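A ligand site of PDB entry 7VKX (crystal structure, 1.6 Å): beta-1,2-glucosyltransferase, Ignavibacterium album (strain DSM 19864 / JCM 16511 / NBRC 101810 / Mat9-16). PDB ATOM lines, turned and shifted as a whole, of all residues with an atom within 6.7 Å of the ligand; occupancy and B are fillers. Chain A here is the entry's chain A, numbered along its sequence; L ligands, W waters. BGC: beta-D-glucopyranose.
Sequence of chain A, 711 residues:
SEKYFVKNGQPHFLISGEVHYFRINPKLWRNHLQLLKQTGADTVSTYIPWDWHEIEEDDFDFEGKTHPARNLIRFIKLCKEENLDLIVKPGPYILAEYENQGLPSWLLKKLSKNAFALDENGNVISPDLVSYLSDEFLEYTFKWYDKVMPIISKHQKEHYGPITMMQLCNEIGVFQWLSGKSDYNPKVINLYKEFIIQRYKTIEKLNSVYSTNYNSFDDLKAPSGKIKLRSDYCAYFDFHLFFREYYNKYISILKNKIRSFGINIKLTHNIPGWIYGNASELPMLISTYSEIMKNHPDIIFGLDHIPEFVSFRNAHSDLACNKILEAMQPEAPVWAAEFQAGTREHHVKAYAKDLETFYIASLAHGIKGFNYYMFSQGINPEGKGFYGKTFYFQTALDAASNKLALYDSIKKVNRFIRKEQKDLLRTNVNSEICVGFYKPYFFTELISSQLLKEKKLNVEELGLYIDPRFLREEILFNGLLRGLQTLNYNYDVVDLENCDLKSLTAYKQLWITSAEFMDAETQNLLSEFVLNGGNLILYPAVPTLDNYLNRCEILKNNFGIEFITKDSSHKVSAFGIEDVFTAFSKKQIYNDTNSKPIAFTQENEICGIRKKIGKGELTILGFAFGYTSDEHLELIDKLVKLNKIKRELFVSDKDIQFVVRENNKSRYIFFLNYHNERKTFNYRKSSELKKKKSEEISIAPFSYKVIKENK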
ATOM      1  N   LEU A  95      -8.757  16.179 -27.919  1.00  0.00           N
ATOM      2  CA  LEU A  95      -8.865  14.864 -27.247  1.00  0.00           C
ATOM      3  C   LEU A  95     -10.144  14.190 -27.739  1.00  0.00           C
ATOM      4  O   LEU A  95     -10.140  13.700 -28.892  1.00  0.00           O
ATOM      5  CB  LEU A  95      -8.775  15.000 -25.705  1.00  0.00           C
ATOM      6  CG  LEU A  95      -8.314  13.754 -24.948  1.00  0.00           C
ATOM      7  CD1 LEU A  95      -7.732  14.133 -23.567  1.00  0.00           C
ATOM      8  CD2 LEU A  95      -9.441  12.769 -24.754  1.00  0.00           C
ATOM      9  N   ALA A  96     -11.258  14.211 -27.000  1.00  0.00           N
ATOM     10  CA  ALA A  96     -12.618  13.812 -27.460  1.00  0.00           C
ATOM     11  C   ALA A  96     -12.633  12.384 -28.011  1.00  0.00           C
ATOM     12  O   ALA A  96     -13.549  12.084 -28.795  1.00  0.00           O
ATOM     13  CB  ALA A  96     -13.115  14.781 -28.498  1.00  0.00           C
ATOM     14  N   GLU A  97     -11.697  11.519 -27.602  1.00  0.00           N
ATOM     15  CA  GLU A  97     -11.528  10.148 -28.161  1.00  0.00           C
ATOM     16  C   GLU A  97     -11.636  10.206 -29.690  1.00  0.00           C
ATOM     17  O   GLU A  97     -12.278   9.327 -30.263  1.00  0.00           O
ATOM     18  CB  GLU A  97     -12.603   9.202 -27.642  1.00  0.00           C
ATOM     19  CG  GLU A  97     -12.475   8.936 -26.167  1.00  0.00           C
ATOM     20  CD  GLU A  97     -13.433   7.858 -25.691  1.00  0.00           C
ATOM     21  OE1 GLU A  97     -14.263   7.274 -26.538  1.00  0.00           O
ATOM     22  OE2 GLU A  97     -13.339   7.559 -24.499  1.00  0.00           O
ATOM     23  N   ASN A 170      -7.410  22.117 -25.337  1.00  0.00           N
ATOM     24  CA  ASN A 170      -8.137  21.103 -24.520  1.00  0.00           C
ATOM     25  C   ASN A 170      -7.173  20.595 -23.459  1.00  0.00           C
ATOM     26  O   ASN A 170      -6.179  19.964 -23.850  1.00  0.00           O
ATOM     27  CB  ASN A 170      -8.730  19.967 -25.357  1.00  0.00           C
ATOM     28  CG  ASN A 170      -9.740  19.192 -24.537  1.00  0.00           C
ATOM     29  OD1 ASN A 170     -10.907  19.576 -24.405  1.00  0.00           O
ATOM     30  ND2 ASN A 170      -9.280  18.123 -23.947  1.00  0.00           N
ATOM     31  N   GLU A 171      -7.502  20.803 -22.165  1.00  0.00           N
ATOM     32  CA  GLU A 171      -6.739  20.241 -21.019  1.00  0.00           C
ATOM     33  C   GLU A 171      -5.252  20.308 -21.314  1.00  0.00           C
ATOM     34  O   GLU A 171      -4.580  19.268 -21.346  1.00  0.00           O
ATOM     35  CB  GLU A 171      -7.244  18.798 -20.743  1.00  0.00           C
ATOM     36  CG  GLU A 171      -8.686  18.668 -20.299  1.00  0.00           C
ATOM     37  CD  GLU A 171      -9.152  17.239 -20.042  1.00  0.00           C
ATOM     38  OE1 GLU A 171      -8.506  16.306 -20.626  1.00  0.00           O
ATOM     39  OE2 GLU A 171     -10.149  17.028 -19.261  1.00  0.00           O
ATOM     40  N   VAL A 174      -2.452  17.486 -20.559  1.00  0.00           N
ATOM     41  CA  VAL A 174      -3.122  16.191 -20.229  1.00  0.00           C
ATOM     42  C   VAL A 174      -2.412  15.069 -20.965  1.00  0.00           C
ATOM     43  O   VAL A 174      -2.223  13.997 -20.350  1.00  0.00           O
ATOM     44  CB  VAL A 174      -4.630  16.179 -20.561  1.00  0.00           C
ATOM     45  CG1 VAL A 174      -4.931  16.133 -22.059  1.00  0.00           C
ATOM     46  CG2 VAL A 174      -5.327  15.032 -19.867  1.00  0.00           C
ATOM     47  N   TRP A 177       0.857  14.354 -19.225  1.00  0.00           N
ATOM     48  CA  TRP A 177       0.508  13.676 -17.946  1.00  0.00           C
ATOM     49  C   TRP A 177       0.157  12.194 -18.206  1.00  0.00           C
ATOM     50  O   TRP A 177       0.782  11.332 -17.552  1.00  0.00           O
ATOM     51  CB  TRP A 177      -0.639  14.448 -17.271  1.00  0.00           C
ATOM     52  CG  TRP A 177      -1.213  13.800 -16.063  1.00  0.00           C
ATOM     53  CD1 TRP A 177      -0.566  13.497 -14.904  1.00  0.00           C
ATOM     54  CD2 TRP A 177      -2.603  13.536 -15.847  1.00  0.00           C
ATOM     55  NE1 TRP A 177      -1.455  12.964 -13.999  1.00  0.00           N
ATOM     56  CE2 TRP A 177      -2.706  12.941 -14.583  1.00  0.00           C
ATOM     57  CE3 TRP A 177      -3.764  13.639 -16.644  1.00  0.00           C
ATOM     58  CZ2 TRP A 177      -3.935  12.524 -14.064  1.00  0.00           C
ATOM     59  CZ3 TRP A 177      -4.974  13.222 -16.129  1.00  0.00           C
ATOM     60  CH2 TRP A 177      -5.050  12.687 -14.852  1.00  0.00           C
ATOM     61  N   LEU A 178      -0.746  11.888 -19.139  1.00  0.00           N
ATOM     62  CA  LEU A 178      -1.176  10.493 -19.407  1.00  0.00           C
ATOM     63  C   LEU A 178      -0.045   9.681 -20.049  1.00  0.00           C
ATOM     64  O   LEU A 178      -0.004   8.485 -19.814  1.00  0.00           O
ATOM     65  CB  LEU A 178      -2.411  10.495 -20.302  1.00  0.00           C
ATOM     66  CG  LEU A 178      -3.640  11.066 -19.625  1.00  0.00           C
ATOM     67  CD1 LEU A 178      -4.747  11.205 -20.636  1.00  0.00           C
ATOM     68  CD2 LEU A 178      -4.102  10.251 -18.421  1.00  0.00           C
ATOM     69  N   ASN A 270     -10.234  24.008 -19.701  1.00  0.00           N
ATOM     70  CA  ASN A 270     -10.884  22.881 -18.983  1.00  0.00           C
ATOM     71  C   ASN A 270      -9.838  22.090 -18.224  1.00  0.00           C
ATOM     72  O   ASN A 270      -8.723  21.936 -18.752  1.00  0.00           O
ATOM     73  CB  ASN A 270     -11.699  22.041 -19.948  1.00  0.00           C
ATOM     74  CG  ASN A 270     -10.963  21.521 -21.156  1.00  0.00           C
ATOM     75  OD1 ASN A 270     -10.015  22.137 -21.656  1.00  0.00           O
ATOM     76  ND2 ASN A 270     -11.403  20.378 -21.656  1.00  0.00           N
ATOM     77  N   ILE A 271     -10.152  21.683 -16.999  1.00  0.00           N
ATOM     78  CA  ILE A 271      -9.147  21.092 -16.075  1.00  0.00           C
ATOM     79  C   ILE A 271      -9.348  19.584 -16.010  1.00  0.00           C
ATOM     80  O   ILE A 271     -10.371  19.126 -15.521  1.00  0.00           O
ATOM     81  CB  ILE A 271      -9.277  21.725 -14.709  1.00  0.00           C
ATOM     82  CG1 ILE A 271      -9.209  23.253 -14.784  1.00  0.00           C
ATOM     83  CG2 ILE A 271      -8.214  21.095 -13.794  1.00  0.00           C
ATOM     84  CD1 ILE A 271      -9.749  23.927 -13.556  1.00  0.00           C
ATOM     85  N   PRO A 272      -8.294  18.821 -16.368  1.00  0.00           N
ATOM     86  CA  PRO A 272      -8.288  17.372 -16.191  1.00  0.00           C
ATOM     87  C   PRO A 272      -7.896  16.943 -14.782  1.00  0.00           C
ATOM     88  O   PRO A 272      -7.455  17.772 -13.964  1.00  0.00           O
ATOM     89  CB  PRO A 272      -7.139  16.925 -17.117  1.00  0.00           C
ATOM     90  CG  PRO A 272      -6.162  18.072 -17.068  1.00  0.00           C
ATOM     91  CD  PRO A 272      -7.014  19.309 -16.913  1.00  0.00           C
ATOM     92  N   GLY A 273      -8.074  15.658 -14.494  1.00  0.00           N
ATOM     93  CA  GLY A 273      -7.431  15.074 -13.330  1.00  0.00           C
ATOM     94  C   GLY A 273      -8.204  13.967 -12.674  1.00  0.00           C
ATOM     95  O   GLY A 273      -7.583  13.269 -11.875  1.00  0.00           O
ATOM     96  N   TRP A 274      -9.480  13.780 -12.968  1.00  0.00           N
ATOM     97  CA  TRP A 274     -10.164  12.603 -12.419  1.00  0.00           C
ATOM     98  C   TRP A 274      -9.635  11.344 -13.103  1.00  0.00           C
ATOM     99  O   TRP A 274      -9.424  11.380 -14.335  1.00  0.00           O
ATOM    100  CB  TRP A 274     -11.672  12.661 -12.602  1.00  0.00           C
ATOM    101  CG  TRP A 274     -12.392  13.671 -11.780  1.00  0.00           C
ATOM    102  CD1 TRP A 274     -12.358  15.041 -11.934  1.00  0.00           C
ATOM    103  CD2 TRP A 274     -13.282  13.402 -10.679  1.00  0.00           C
ATOM    104  NE1 TRP A 274     -13.189  15.617 -11.035  1.00  0.00           N
ATOM    105  CE2 TRP A 274     -13.789  14.657 -10.261  1.00  0.00           C
ATOM    106  CE3 TRP A 274     -13.708  12.235 -10.006  1.00  0.00           C
ATOM    107  CZ2 TRP A 274     -14.700  14.742  -9.212  1.00  0.00           C
ATOM    108  CZ3 TRP A 274     -14.586  12.339  -8.953  1.00  0.00           C
ATOM    109  CH2 TRP A 274     -15.108  13.578  -8.608  1.00  0.00           C
ATOM    110  N   ILE A 275      -9.535  10.259 -12.357  1.00  0.00           N
ATOM    111  CA  ILE A 275      -9.232   8.921 -12.920  1.00  0.00           C
ATOM    112  C   ILE A 275      -9.768   7.889 -11.944  1.00  0.00           C
ATOM    113  O   ILE A 275      -9.610   8.029 -10.747  1.00  0.00           O
ATOM    114  CB  ILE A 275      -7.726   8.787 -13.274  1.00  0.00           C
ATOM    115  CG1 ILE A 275      -7.472   7.587 -14.191  1.00  0.00           C
ATOM    116  CG2 ILE A 275      -6.855   8.791 -12.037  1.00  0.00           C
ATOM    117  CD1 ILE A 275      -6.069   7.489 -14.724  1.00  0.00           C
ATOM    118  N   TYR A 276     -10.408   6.866 -12.462  1.00  0.00           N
ATOM    119  CA  TYR A 276     -11.024   5.762 -11.680  1.00  0.00           C
ATOM    120  C   TYR A 276     -12.018   6.290 -10.658  1.00  0.00           C
ATOM    121  O   TYR A 276     -12.243   5.606  -9.642  1.00  0.00           O
ATOM    122  CB  TYR A 276      -9.901   4.962 -10.994  1.00  0.00           C
ATOM    123  CG  TYR A 276      -8.793   4.511 -11.920  1.00  0.00           C
ATOM    124  CD1 TYR A 276      -9.093   3.890 -13.137  1.00  0.00           C
ATOM    125  CD2 TYR A 276      -7.462   4.743 -11.622  1.00  0.00           C
ATOM    126  CE1 TYR A 276      -8.107   3.486 -14.019  1.00  0.00           C
ATOM    127  CE2 TYR A 276      -6.462   4.303 -12.469  1.00  0.00           C
ATOM    128  CZ  TYR A 276      -6.778   3.673 -13.662  1.00  0.00           C
ATOM    129  OH  TYR A 276      -5.792   3.313 -14.552  1.00  0.00           O
ATOM    130  N   ASP A 304     -13.387  19.333 -15.258  1.00  0.00           N
ATOM    131  CA  ASP A 304     -13.865  18.146 -16.007  1.00  0.00           C
ATOM    132  C   ASP A 304     -14.109  17.061 -14.982  1.00  0.00           C
ATOM    133  O   ASP A 304     -13.120  16.391 -14.564  1.00  0.00           O
ATOM    134  CB  ASP A 304     -12.845  17.786 -17.107  1.00  0.00           C
ATOM    135  CG  ASP A 304     -12.709  18.886 -18.169  1.00  0.00           C
ATOM    136  OD1 ASP A 304     -13.569  19.783 -18.178  1.00  0.00           O
ATOM    137  OD2 ASP A 304     -11.748  18.820 -18.954  1.00  0.00           O
ATOM    138  N   HIS A 305     -15.339  16.943 -14.494  1.00  0.00           N
ATOM    139  CA  HIS A 305     -15.682  16.026 -13.394  1.00  0.00           C
ATOM    140  C   HIS A 305     -16.111  14.667 -13.940  1.00  0.00           C
ATOM    141  O   HIS A 305     -17.081  14.591 -14.698  1.00  0.00           O
ATOM    142  CB  HIS A 305     -16.771  16.605 -12.514  1.00  0.00           C
ATOM    143  CG  HIS A 305     -16.381  17.664 -11.539  1.00  0.00           C
ATOM    144  ND1 HIS A 305     -15.093  17.822 -11.012  1.00  0.00           N
ATOM    145  CD2 HIS A 305     -17.163  18.619 -10.978  1.00  0.00           C
ATOM    146  CE1 HIS A 305     -15.146  18.753 -10.081  1.00  0.00           C
ATOM    147  NE2 HIS A 305     -16.407  19.292 -10.066  1.00  0.00           N
ATOM    148  N   ILE A 306     -15.368  13.603 -13.580  1.00  0.00           N
ATOM    149  CA  ILE A 306     -15.652  12.204 -13.992  1.00  0.00           C
ATOM    150  C   ILE A 306     -15.766  11.313 -12.760  1.00  0.00           C
ATOM    151  O   ILE A 306     -14.904  10.469 -12.538  1.00  0.00           O
ATOM    152  CB  ILE A 306     -14.578  11.656 -14.965  1.00  0.00           C
ATOM    153  CG1 ILE A 306     -14.140  12.702 -15.980  1.00  0.00           C
ATOM    154  CG2 ILE A 306     -15.084  10.393 -15.678  1.00  0.00           C
ATOM    155  CD1 ILE A 306     -13.060  12.229 -16.935  1.00  0.00           C
ATOM    156  N   GLU A 308     -17.833   8.705 -12.063  1.00  0.00           N
ATOM    157  CA  GLU A 308     -18.103   7.279 -12.444  1.00  0.00           C
ATOM    158  C   GLU A 308     -19.153   6.647 -11.557  1.00  0.00           C
ATOM    159  O   GLU A 308     -19.959   5.872 -12.106  1.00  0.00           O
ATOM    160  CB  GLU A 308     -16.862   6.398 -12.419  1.00  0.00           C
ATOM    161  CG  GLU A 308     -15.773   6.910 -13.340  1.00  0.00           C
ATOM    162  CD  GLU A 308     -14.524   6.057 -13.552  1.00  0.00           C
ATOM    163  OE1 GLU A 308     -14.442   5.056 -12.825  1.00  0.00           O
ATOM    164  OE2 GLU A 308     -13.659   6.444 -14.382  1.00  0.00           O
ATOM    165  N   GLU A 338     -16.827  19.998 -18.396  1.00  0.00           N
ATOM    166  CA  GLU A 338     -17.287  18.630 -18.727  1.00  0.00           C
ATOM    167  C   GLU A 338     -17.861  18.017 -17.470  1.00  0.00           C
ATOM    168  O   GLU A 338     -17.099  17.869 -16.450  1.00  0.00           O
ATOM    169  CB  GLU A 338     -16.127  17.790 -19.256  1.00  0.00           C
ATOM    170  CG  GLU A 338     -15.457  18.414 -20.492  1.00  0.00           C
ATOM    171  CD  GLU A 338     -14.217  17.718 -21.017  1.00  0.00           C
ATOM    172  OE1 GLU A 338     -13.924  16.602 -20.544  1.00  0.00           O
ATOM    173  OE2 GLU A 338     -13.490  18.307 -21.826  1.00  0.00           O
ATOM    174  N   ARG A 344     -17.629   7.405 -20.790  1.00  0.00           N
ATOM    175  CA  ARG A 344     -16.694   7.248 -21.906  1.00  0.00           C
ATOM    176  C   ARG A 344     -16.322   5.773 -22.169  1.00  0.00           C
ATOM    177  O   ARG A 344     -15.787   5.480 -23.259  1.00  0.00           O
ATOM    178  CB  ARG A 344     -15.409   8.018 -21.625  1.00  0.00           C
ATOM    179  CG  ARG A 344     -14.666   7.530 -20.390  1.00  0.00           C
ATOM    180  CD  ARG A 344     -13.579   8.513 -20.031  1.00  0.00           C
ATOM    181  NE  ARG A 344     -12.851   8.164 -18.806  1.00  0.00           N
ATOM    182  CZ  ARG A 344     -11.717   8.727 -18.402  1.00  0.00           C
ATOM    183  NH1 ARG A 344     -11.113   9.646 -19.147  1.00  0.00           N
ATOM    184  NH2 ARG A 344     -11.170   8.357 -17.273  1.00  0.00           N
ATOM    185  N   LEU A 451       0.669   9.101 -12.419  1.00  0.00           N
ATOM    186  CA  LEU A 451       0.776   8.683 -13.862  1.00  0.00           C
ATOM    187  C   LEU A 451       2.246   8.633 -14.320  1.00  0.00           C
ATOM    188  O   LEU A 451       2.513   8.052 -15.404  1.00  0.00           O
ATOM    189  CB  LEU A 451      -0.014   9.626 -14.765  1.00  0.00           C
ATOM    190  CG  LEU A 451      -1.529   9.406 -14.906  1.00  0.00           C
ATOM    191  CD1 LEU A 451      -1.823   8.175 -15.752  1.00  0.00           C
ATOM    192  CD2 LEU A 451      -2.217   9.273 -13.583  1.00  0.00           C
HETATM  193  C2  BGC L   1      -9.765  13.174 -19.701  1.00  0.00           C
HETATM  194  C3  BGC L   1      -9.295  13.789 -18.444  1.00  0.00           C
HETATM  195  C4  BGC L   1      -9.004  12.735 -17.399  1.00  0.00           C
HETATM  196  C5  BGC L   1      -8.043  11.679 -17.950  1.00  0.00           C
HETATM  197  C6  BGC L   1      -7.759  10.486 -17.066  1.00  0.00           C
HETATM  198  C1  BGC L   1      -8.710  12.173 -20.151  1.00  0.00           C
HETATM  199  O1  BGC L   1      -9.098  11.444 -21.319  1.00  0.00           O
HETATM  200  O2  BGC L   1     -10.013  14.162 -20.721  1.00  0.00           O
HETATM  201  O3  BGC L   1     -10.272  14.663 -17.869  1.00  0.00           O
HETATM  202  O4  BGC L   1      -8.516  13.201 -16.111  1.00  0.00           O
HETATM  203  O5  BGC L   1      -8.608  11.163 -19.145  1.00  0.00           O
HETATM  204  O6  BGC L   1      -8.937   9.892 -16.492  1.00  0.00           O
HETATM  205  O   HOH W   1     -11.678  10.679 -21.829  1.00  0.00           O
HETATM  206  O   HOH W   2     -11.287  16.786 -22.304  1.00  0.00           O
HETATM  207  O   HOH W   3     -12.804  14.149 -20.827  1.00  0.00           O
HETATM  208  O   HOH W   4     -11.041  14.788 -15.194  1.00  0.00           O
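The backbone NH (N) of Gly 273 sits at hydrogen-bond distance from an oxygen (O4) of the ligand. An oxygen (O6) of the ligand sits at hydrogen-bond distance from the backbone carbonyl oxygen (O) of Trp 274. O4 of the ligand is in hydrogen-bond range of N of Trp 274 (3.3 Å). NH2 of Arg 344 lies within hydrogen-bond range of O6 of the ligand. OE1 of Glu 171 lies within hydrogen-bond range of O2 of the ligand.
NE1 of Trp 274 lies within hydrogen-bond range of ND1 of His 305 (2.9 Å). The side-chain carboxylate (OE2) of Glu 171 lies close to the side-chain carboxylate (OD2) of Asp 304 (2.4 Å). OD1 of Asn 270 is in hydrogen-bond range of N of Glu 171, at 2.9 Å.
Merely in contact with the ligand: Leu 95, Trp 177, Leu 178, Pro 272, Ile 275 and Ile 306. Hydrophobic or aromatic side chains within 4 Å of the ligand: Leu 95, Trp 177, Leu 178, Pro 272, Ile 275 and Ile 306. Of the 22 residues printed, 10 come within 4 Å of the ligand.
Water W1 lies within hydrogen-bond range of an oxygen (O1) of the ligand (2.7 Å) and the guanidinium group of Arg 344 (2.9 Å). Water W4 lies within hydrogen-bond range of the backbone carbonyl oxygen (O) of Asp 304, an oxygen (O3) of the ligand, the backbone NH (N) of Trp 274 and the backbone NH (N) of Gly 273. Water W3 lies within hydrogen-bond range of the side-chain carboxylate of Glu 338 (2.7 Å) and an oxygen (O2) of the ligand (2.8 Å). Water W2 lies within hydrogen-bond range of the side-chain carboxylate (OE2) of Glu 338 (2.7 Å), the side-chain amide nitrogen (ND2) of Asn 170 (2.9 Å), the side-chain carboxylate (OE2) of Glu 171 (3.3 Å) and an oxygen (O2) of the ligand (3.3 Å).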
